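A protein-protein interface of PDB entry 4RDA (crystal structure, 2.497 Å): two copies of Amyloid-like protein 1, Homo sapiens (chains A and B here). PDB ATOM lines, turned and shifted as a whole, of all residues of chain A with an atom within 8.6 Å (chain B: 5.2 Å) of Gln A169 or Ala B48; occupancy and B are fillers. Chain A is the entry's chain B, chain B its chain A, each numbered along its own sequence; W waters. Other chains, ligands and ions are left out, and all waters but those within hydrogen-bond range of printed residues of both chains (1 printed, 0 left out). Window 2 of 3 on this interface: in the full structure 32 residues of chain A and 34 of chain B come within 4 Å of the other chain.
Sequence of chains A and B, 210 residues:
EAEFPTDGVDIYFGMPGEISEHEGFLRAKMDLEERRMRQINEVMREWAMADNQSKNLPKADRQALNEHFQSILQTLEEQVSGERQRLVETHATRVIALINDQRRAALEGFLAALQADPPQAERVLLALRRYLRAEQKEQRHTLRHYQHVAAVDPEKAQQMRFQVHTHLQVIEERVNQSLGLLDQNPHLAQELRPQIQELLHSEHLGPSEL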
ATOM      1  N   GLN A 139     -20.493  -6.978  26.596  1.00  0.00           N
ATOM      2  CA  GLN A 139     -21.238  -6.032  25.793  1.00  0.00           C
ATOM      3  C   GLN A 139     -21.222  -6.438  24.321  1.00  0.00           C
ATOM      4  O   GLN A 139     -22.291  -6.485  23.698  1.00  0.00           O
ATOM      5  CB  GLN A 139     -20.698  -4.614  25.972  1.00  0.00           C
ATOM      6  CG  GLN A 139     -21.525  -3.590  25.269  1.00  0.00           C
ATOM      7  CD  GLN A 139     -20.755  -2.339  25.025  1.00  0.00           C
ATOM      8  OE1 GLN A 139     -19.573  -2.265  25.353  1.00  0.00           O
ATOM      9  NE2 GLN A 139     -21.405  -1.337  24.439  1.00  0.00           N
ATOM     10  N   THR A 142     -23.501  -9.437  23.802  1.00  0.00           N
ATOM     11  CA  THR A 142     -24.921  -9.087  23.864  1.00  0.00           C
ATOM     12  C   THR A 142     -25.400  -8.445  22.565  1.00  0.00           C
ATOM     13  O   THR A 142     -26.436  -8.830  22.019  1.00  0.00           O
ATOM     14  CB  THR A 142     -25.208  -8.140  25.044  1.00  0.00           C
ATOM     15  OG1 THR A 142     -24.824  -8.783  26.268  1.00  0.00           O
ATOM     16  CG2 THR A 142     -26.685  -7.820  25.102  1.00  0.00           C
ATOM     17  N   PHE A 162     -36.158  -5.324  24.149  1.00  0.00           N
ATOM     18  CA  PHE A 162     -36.166  -4.583  25.397  1.00  0.00           C
ATOM     19  C   PHE A 162     -35.187  -5.178  26.415  1.00  0.00           C
ATOM     20  O   PHE A 162     -34.517  -4.437  27.150  1.00  0.00           O
ATOM     21  CB  PHE A 162     -37.585  -4.530  25.973  1.00  0.00           C
ATOM     22  CG  PHE A 162     -37.724  -3.625  27.180  1.00  0.00           C
ATOM     23  CD1 PHE A 162     -37.961  -2.277  27.025  1.00  0.00           C
ATOM     24  CD2 PHE A 162     -37.612  -4.134  28.465  1.00  0.00           C
ATOM     25  CE1 PHE A 162     -38.069  -1.454  28.117  1.00  0.00           C
ATOM     26  CE2 PHE A 162     -37.730  -3.320  29.551  1.00  0.00           C
ATOM     27  CZ  PHE A 162     -37.956  -1.975  29.383  1.00  0.00           C
ATOM     28  N   GLN A 163     -35.107  -6.508  26.463  1.00  0.00           N
ATOM     29  CA  GLN A 163     -34.151  -7.199  27.333  1.00  0.00           C
ATOM     30  C   GLN A 163     -32.715  -6.780  27.017  1.00  0.00           C
ATOM     31  O   GLN A 163     -31.899  -6.588  27.919  1.00  0.00           O
ATOM     32  CB  GLN A 163     -34.279  -8.716  27.196  1.00  0.00           C
ATOM     33  CG  GLN A 163     -35.674  -9.281  27.455  1.00  0.00           C
ATOM     34  CD  GLN A 163     -35.883 -10.659  26.813  1.00  0.00           C
ATOM     35  N   VAL A 164     -32.398  -6.640  25.738  1.00  0.00           N
ATOM     36  CA  VAL A 164     -31.034  -6.284  25.345  1.00  0.00           C
ATOM     37  C   VAL A 164     -30.719  -4.874  25.844  1.00  0.00           C
ATOM     38  O   VAL A 164     -29.681  -4.645  26.468  1.00  0.00           O
ATOM     39  CB  VAL A 164     -30.837  -6.401  23.796  1.00  0.00           C
ATOM     40  CG1 VAL A 164     -29.454  -5.929  23.366  1.00  0.00           C
ATOM     41  CG2 VAL A 164     -31.076  -7.835  23.349  1.00  0.00           C
ATOM     42  N   HIS A 165     -31.630  -3.944  25.571  1.00  0.00           N
ATOM     43  CA  HIS A 165     -31.601  -2.587  26.137  1.00  0.00           C
ATOM     44  C   HIS A 165     -31.304  -2.603  27.640  1.00  0.00           C
ATOM     45  O   HIS A 165     -30.344  -1.966  28.100  1.00  0.00           O
ATOM     46  CB  HIS A 165     -32.940  -1.900  25.872  1.00  0.00           C
ATOM     47  CG  HIS A 165     -33.073  -0.539  26.485  1.00  0.00           C
ATOM     48  ND1 HIS A 165     -32.286   0.560  26.397  1.00  0.00           N
ATOM     49  CD2 HIS A 165     -34.161  -0.172  27.256  1.00  0.00           C
ATOM     50  CE1 HIS A 165     -32.905   1.558  27.116  1.00  0.00           C
ATOM     51  NE2 HIS A 165     -34.034   1.092  27.617  1.00  0.00           N
ATOM     52  N   THR A 166     -32.126  -3.333  28.395  1.00  0.00           N
ATOM     53  CA  THR A 166     -31.918  -3.480  29.830  1.00  0.00           C
ATOM     54  C   THR A 166     -30.526  -4.053  30.158  1.00  0.00           C
ATOM     55  O   THR A 166     -29.811  -3.538  31.029  1.00  0.00           O
ATOM     56  CB  THR A 166     -32.981  -4.399  30.453  1.00  0.00           C
ATOM     57  OG1 THR A 166     -34.288  -3.891  30.164  1.00  0.00           O
ATOM     58  CG2 THR A 166     -32.792  -4.497  31.957  1.00  0.00           C
ATOM     59  N   HIS A 167     -30.140  -5.122  29.454  1.00  0.00           N
ATOM     60  CA  HIS A 167     -28.856  -5.761  29.713  1.00  0.00           C
ATOM     61  C   HIS A 167     -27.688  -4.793  29.478  1.00  0.00           C
ATOM     62  O   HIS A 167     -26.794  -4.695  30.309  1.00  0.00           O
ATOM     63  CB  HIS A 167     -28.705  -7.011  28.857  1.00  0.00           C
ATOM     64  CG  HIS A 167     -27.502  -7.836  29.201  1.00  0.00           C
ATOM     65  ND1 HIS A 167     -27.286  -9.095  28.679  1.00  0.00           N
ATOM     66  CD2 HIS A 167     -26.448  -7.576  30.012  1.00  0.00           C
ATOM     67  CE1 HIS A 167     -26.151  -9.569  29.153  1.00  0.00           C
ATOM     68  NE2 HIS A 167     -25.625  -8.668  29.965  1.00  0.00           N
ATOM     69  N   LEU A 168     -27.702  -4.069  28.365  1.00  0.00           N
ATOM     70  CA  LEU A 168     -26.682  -3.058  28.110  1.00  0.00           C
ATOM     71  C   LEU A 168     -26.607  -1.985  29.190  1.00  0.00           C
ATOM     72  O   LEU A 168     -25.524  -1.480  29.465  1.00  0.00           O
ATOM     73  CB  LEU A 168     -26.925  -2.391  26.755  1.00  0.00           C
ATOM     74  CG  LEU A 168     -26.806  -3.326  25.556  1.00  0.00           C
ATOM     75  CD1 LEU A 168     -27.078  -2.642  24.231  1.00  0.00           C
ATOM     76  CD2 LEU A 168     -25.413  -3.969  25.567  1.00  0.00           C
ATOM     77  N   GLN A 169     -27.742  -1.617  29.790  1.00  0.00           N
ATOM     78  CA  GLN A 169     -27.743  -0.566  30.816  1.00  0.00           C
ATOM     79  C   GLN A 169     -27.107  -1.103  32.067  1.00  0.00           C
ATOM     80  O   GLN A 169     -26.428  -0.377  32.799  1.00  0.00           O
ATOM     81  CB  GLN A 169     -29.159  -0.082  31.160  1.00  0.00           C
ATOM     82  CG  GLN A 169     -29.836   0.795  30.142  1.00  0.00           C
ATOM     83  CD  GLN A 169     -31.253   1.167  30.578  1.00  0.00           C
ATOM     84  OE1 GLN A 169     -32.171   0.348  30.474  1.00  0.00           O
ATOM     85  NE2 GLN A 169     -31.431   2.396  31.090  1.00  0.00           N
ATOM     86  N   VAL A 170     -27.372  -2.381  32.330  1.00  0.00           N
ATOM     87  CA  VAL A 170     -26.830  -3.019  33.515  1.00  0.00           C
ATOM     88  C   VAL A 170     -25.295  -3.037  33.431  1.00  0.00           C
ATOM     89  O   VAL A 170     -24.617  -2.690  34.397  1.00  0.00           O
ATOM     90  CB  VAL A 170     -27.404  -4.432  33.686  1.00  0.00           C
ATOM     91  CG1 VAL A 170     -26.530  -5.276  34.595  1.00  0.00           C
ATOM     92  CG2 VAL A 170     -28.828  -4.355  34.210  1.00  0.00           C
ATOM     93  N   ILE A 171     -24.752  -3.393  32.270  1.00  0.00           N
ATOM     94  CA  ILE A 171     -23.304  -3.435  32.103  1.00  0.00           C
ATOM     95  C   ILE A 171     -22.771  -2.032  32.355  1.00  0.00           C
ATOM     96  O   ILE A 171     -21.848  -1.849  33.142  1.00  0.00           O
ATOM     97  CB  ILE A 171     -22.872  -3.958  30.680  1.00  0.00           C
ATOM     98  CG1 ILE A 171     -23.427  -5.359  30.426  1.00  0.00           C
ATOM     99  CG2 ILE A 171     -21.337  -3.928  30.496  1.00  0.00           C
ATOM    100  CD1 ILE A 171     -23.168  -5.900  29.021  1.00  0.00           C
ATOM    101  N   GLU A 172     -23.392  -1.044  31.725  1.00  0.00           N
ATOM    102  CA  GLU A 172     -22.983   0.366  31.850  1.00  0.00           C
ATOM    103  C   GLU A 172     -22.985   0.881  33.297  1.00  0.00           C
ATOM    104  O   GLU A 172     -22.083   1.601  33.712  1.00  0.00           O
ATOM    105  CB  GLU A 172     -23.890   1.245  31.000  1.00  0.00           C
ATOM    106  CG  GLU A 172     -23.299   2.594  30.709  1.00  0.00           C
ATOM    107  CD  GLU A 172     -22.030   2.480  29.897  1.00  0.00           C
ATOM    108  OE1 GLU A 172     -22.089   1.846  28.821  1.00  0.00           O
ATOM    109  OE2 GLU A 172     -20.978   3.002  30.340  1.00  0.00           O
ATOM    110  N   GLU A 173     -24.002   0.501  34.055  1.00  0.00           N
ATOM    111  CA  GLU A 173     -24.087   0.825  35.471  1.00  0.00           C
ATOM    112  C   GLU A 173     -22.986   0.171  36.296  1.00  0.00           C
ATOM    113  O   GLU A 173     -22.412   0.798  37.174  1.00  0.00           O
ATOM    114  CB  GLU A 173     -25.454   0.409  36.020  1.00  0.00           C
ATOM    115  CG  GLU A 173     -26.588   1.390  35.700  1.00  0.00           C
ATOM    116  CD  GLU A 173     -27.955   0.708  35.624  1.00  0.00           C
ATOM    117  OE1 GLU A 173     -28.865   1.303  35.011  1.00  0.00           O
ATOM    118  OE2 GLU A 173     -28.125  -0.414  36.162  1.00  0.00           O
ATOM    119  N   ARG A 174     -22.701  -1.099  36.029  1.00  0.00           N
ATOM    120  CA  ARG A 174     -21.590  -1.779  36.697  1.00  0.00           C
ATOM    121  C   ARG A 174     -20.252  -1.098  36.438  1.00  0.00           C
ATOM    122  O   ARG A 174     -19.491  -0.851  37.371  1.00  0.00           O
ATOM    123  CB  ARG A 174     -21.506  -3.234  36.262  1.00  0.00           C
ATOM    124  CG  ARG A 174     -22.102  -4.182  37.249  1.00  0.00           C
ATOM    125  CD  ARG A 174     -21.478  -5.549  37.082  1.00  0.00           C
ATOM    126  NE  ARG A 174     -21.334  -5.943  35.684  1.00  0.00           N
ATOM    127  CZ  ARG A 174     -22.258  -6.601  34.986  1.00  0.00           C
ATOM    128  NH1 ARG A 174     -23.414  -6.936  35.552  1.00  0.00           N
ATOM    129  NH2 ARG A 174     -22.018  -6.933  33.718  1.00  0.00           N
ATOM    130  N   VAL A 175     -19.963  -0.803  35.172  1.00  0.00           N
ATOM    131  CA  VAL A 175     -18.729  -0.108  34.826  1.00  0.00           C
ATOM    132  C   VAL A 175     -18.606   1.230  35.542  1.00  0.00           C
ATOM    133  O   VAL A 175     -17.575   1.506  36.152  1.00  0.00           O
ATOM    134  CB  VAL A 175     -18.614   0.147  33.320  1.00  0.00           C
ATOM    135  CG1 VAL A 175     -17.377   1.011  33.017  1.00  0.00           C
ATOM    136  CG2 VAL A 175     -18.576  -1.162  32.558  1.00  0.00           C
ATOM    137  N   ASN A 176     -19.645   2.062  35.471  1.00  0.00           N
ATOM    138  CA  ASN A 176     -19.611   3.356  36.156  1.00  0.00           C
ATOM    139  C   ASN A 176     -19.363   3.203  37.651  1.00  0.00           C
ATOM    140  O   ASN A 176     -18.539   3.906  38.219  1.00  0.00           O
ATOM    141  CB  ASN A 176     -20.912   4.143  35.935  1.00  0.00           C
ATOM    142  CG  ASN A 176     -21.085   4.606  34.496  1.00  0.00           C
ATOM    143  OD1 ASN A 176     -20.112   4.814  33.769  1.00  0.00           O
ATOM    144  ND2 ASN A 176     -22.337   4.762  34.080  1.00  0.00           N
ATOM    145  N   VAL B  43     -28.090   3.542  19.001  1.00  0.00           N
ATOM    146  CA  VAL B  43     -29.518   3.658  19.288  1.00  0.00           C
ATOM    147  C   VAL B  43     -29.841   3.224  20.729  1.00  0.00           C
ATOM    148  O   VAL B  43     -30.606   3.882  21.426  1.00  0.00           O
ATOM    149  CB  VAL B  43     -30.360   2.839  18.319  1.00  0.00           C
ATOM    150  CG1 VAL B  43     -31.832   2.876  18.744  1.00  0.00           C
ATOM    151  CG2 VAL B  43     -30.191   3.358  16.916  1.00  0.00           C
ATOM    152  N   MET B  44     -29.229   2.131  21.171  1.00  0.00           N
ATOM    153  CA  MET B  44     -29.408   1.638  22.539  1.00  0.00           C
ATOM    154  C   MET B  44     -28.960   2.646  23.580  1.00  0.00           C
ATOM    155  O   MET B  44     -29.530   2.711  24.665  1.00  0.00           O
ATOM    156  CB  MET B  44     -28.628   0.325  22.743  1.00  0.00           C
ATOM    157  CG  MET B  44     -29.190  -0.858  21.999  1.00  0.00           C
ATOM    158  SD  MET B  44     -30.745  -1.372  22.711  1.00  0.00           S
ATOM    159  CE  MET B  44     -31.177  -2.680  21.548  1.00  0.00           C
ATOM    160  N   ARG B  45     -27.903   3.394  23.265  1.00  0.00           N
ATOM    161  CA  ARG B  45     -27.385   4.378  24.200  1.00  0.00           C
ATOM    162  C   ARG B  45     -28.352   5.562  24.327  1.00  0.00           C
ATOM    163  O   ARG B  45     -28.646   5.992  25.442  1.00  0.00           O
ATOM    164  CB  ARG B  45     -25.984   4.857  23.792  1.00  0.00           C
ATOM    165  CG  ARG B  45     -24.843   4.133  24.526  1.00  0.00           C
ATOM    166  CD  ARG B  45     -23.462   4.582  24.033  1.00  0.00           C
ATOM    167  N   GLU B  46     -28.860   6.061  23.199  1.00  0.00           N
ATOM    168  CA  GLU B  46     -29.877   7.107  23.226  1.00  0.00           C
ATOM    169  C   GLU B  46     -31.098   6.667  24.023  1.00  0.00           C
ATOM    170  O   GLU B  46     -31.639   7.439  24.816  1.00  0.00           O
ATOM    171  CB  GLU B  46     -30.315   7.495  21.820  1.00  0.00           C
ATOM    172  CG  GLU B  46     -29.266   8.202  21.017  1.00  0.00           C
ATOM    173  CD  GLU B  46     -29.666   8.308  19.562  1.00  0.00           C
ATOM    174  OE1 GLU B  46     -30.778   8.842  19.304  1.00  0.00           O
ATOM    175  OE2 GLU B  46     -28.887   7.837  18.690  1.00  0.00           O
ATOM    176  N   TRP B  47     -31.534   5.430  23.808  1.00  0.00           N
ATOM    177  CA  TRP B  47     -32.688   4.916  24.529  1.00  0.00           C
ATOM    178  C   TRP B  47     -32.427   4.997  26.029  1.00  0.00           C
ATOM    179  O   TRP B  47     -33.270   5.482  26.792  1.00  0.00           O
ATOM    180  CB  TRP B  47     -32.988   3.484  24.098  1.00  0.00           C
ATOM    181  CG  TRP B  47     -34.306   2.919  24.560  1.00  0.00           C
ATOM    182  CD1 TRP B  47     -35.250   3.535  25.331  1.00  0.00           C
ATOM    183  CD2 TRP B  47     -34.830   1.621  24.244  1.00  0.00           C
ATOM    184  NE1 TRP B  47     -36.326   2.699  25.520  1.00  0.00           N
ATOM    185  CE2 TRP B  47     -36.087   1.520  24.867  1.00  0.00           C
ATOM    186  CE3 TRP B  47     -34.355   0.548  23.490  1.00  0.00           C
ATOM    187  CZ2 TRP B  47     -36.876   0.365  24.760  1.00  0.00           C
ATOM    188  CZ3 TRP B  47     -35.142  -0.595  23.385  1.00  0.00           C
ATOM    189  CH2 TRP B  47     -36.384  -0.676  24.015  1.00  0.00           C
ATOM    190  N   ALA B  48     -31.243   4.544  26.434  1.00  0.00           N
ATOM    191  CA  ALA B  48     -30.827   4.549  27.835  1.00  0.00           C
ATOM    192  C   ALA B  48     -30.808   5.949  28.424  1.00  0.00           C
ATOM    193  O   ALA B  48     -31.212   6.154  29.560  1.00  0.00           O
ATOM    194  CB  ALA B  48     -29.445   3.915  27.983  1.00  0.00           C
ATOM    195  N   MET B  49     -30.312   6.896  27.635  1.00  0.00           N
ATOM    196  CA  MET B  49     -30.113   8.256  28.082  1.00  0.00           C
ATOM    197  C   MET B  49     -31.461   8.973  28.236  1.00  0.00           C
ATOM    198  O   MET B  49     -31.672   9.695  29.199  1.00  0.00           O
ATOM    199  CB  MET B  49     -29.196   8.990  27.110  1.00  0.00           C
ATOM    200  CG  MET B  49     -28.287  10.011  27.776  1.00  0.00           C
ATOM    201  SD  MET B  49     -27.091  10.710  26.624  1.00  0.00           S
ATOM    202  N   ALA B  50     -32.377   8.741  27.302  1.00  0.00           N
ATOM    203  CA  ALA B  50     -33.752   9.213  27.447  1.00  0.00           C
ATOM    204  C   ALA B  50     -34.423   8.572  28.656  1.00  0.00           C
ATOM    205  O   ALA B  50     -35.200   9.213  29.367  1.00  0.00           O
ATOM    206  CB  ALA B  50     -34.552   8.930  26.189  1.00  0.00           C
ATOM    207  N   ASP B  51     -34.103   7.308  28.897  1.00  0.00           N
ATOM    208  CA  ASP B  51     -34.683   6.564  30.007  1.00  0.00           C
ATOM    209  C   ASP B  51     -34.233   7.088  31.371  1.00  0.00           C
ATOM    210  O   ASP B  51     -34.996   7.065  32.342  1.00  0.00           O
ATOM    211  CB  ASP B  51     -34.326   5.087  29.875  1.00  0.00           C
ATOM    212  CG  ASP B  51     -35.537   4.197  29.920  1.00  0.00           C
ATOM    213  OD1 ASP B  51     -36.324   4.333  30.886  1.00  0.00           O
ATOM    214  OD2 ASP B  51     -35.706   3.376  28.988  1.00  0.00           O
ATOM    215  N   ASN B  52     -32.992   7.554  31.436  1.00  0.00           N
ATOM    216  CA  ASN B  52     -32.406   8.002  32.692  1.00  0.00           C
ATOM    217  C   ASN B  52     -33.000   9.316  33.184  1.00  0.00           C
ATOM    218  O   ASN B  52     -33.107   9.543  34.389  1.00  0.00           O
ATOM    219  CB  ASN B  52     -30.892   8.144  32.548  1.00  0.00           C
ATOM    220  CG  ASN B  52     -30.182   6.804  32.543  1.00  0.00           C
ATOM    221  OD1 ASN B  52     -30.541   5.898  33.298  1.00  0.00           O
ATOM    222  ND2 ASN B  52     -29.169   6.667  31.686  1.00  0.00           N
HETATM  223  O   HOH W   1     -29.335   0.480  26.569  1.00  0.00           O
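The indole nitrogen of Trp B47 lies close to a ring nitrogen (NE2) of His A165 (3.5 Å). A ring nitrogen (NE2) of His A165 lies within hydrogen-bond range of the side-chain carboxylate of Asp B51 (3.1 Å).
ND2 of Asn B52 lies within hydrogen-bond range of O of Ala B48. The backbone carbonyl oxygen (O) of Phe A162 is in hydrogen-bond range of the side-chain hydroxyl (OG1) of Thr A166 (3.1 Å). A ring nitrogen (NE2) of His A165 sits at hydrogen-bond distance from the side-chain amide oxygen (OE1) of Gln A169.
CD1 of Phe A162 touches CZ2 of Trp B47 (3.6 Å). His A165 touches Met B44 (CA to SD, 3.7 Å). His A165 touches Ala B48 (CE1 to N, 3.5 Å). Leu A168 touches Met B44. Gln A169 touches Ala B48 (CG to CB, 3.8 Å).
Of chain B, only Ala B48 comes within 4 Å of Gln A169. Printed residues of chain B within 4 Å of Leu A168: Met B44. Of the printed residues of chain A, Asp B51 touches His A165. The nearest residue of chain B that does not touch Gln A169 is Asp B51 (4.1 Å). The nearest printed residue of chain A that does not touch Met B44 is Val A164 (4.1 Å).
Of the 10 printed residues of chain B, 4 touch a printed residue of chain A. Printed residues of chain B that touch a printed residue of chain A: Met B44, Trp B47, Ala B48 and Asp B51. Hydrophobic or aromatic side chains of chain B that line the printed part of chain A: Met B44, Trp B47 and Ala B48. Along chain B the printed residues that touch a printed residue of chain A span positions 44 to 51. Among the printed residues, 7 pairs touch across the chains. Among the printed residues, no Asp or Glu carboxylate lies within 4 Å of a Lys or Arg side-chain nitrogen of the other chain.
No position is printed for both chains.
Water W1 bridges O of Met B44 and ND1 of His A165.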
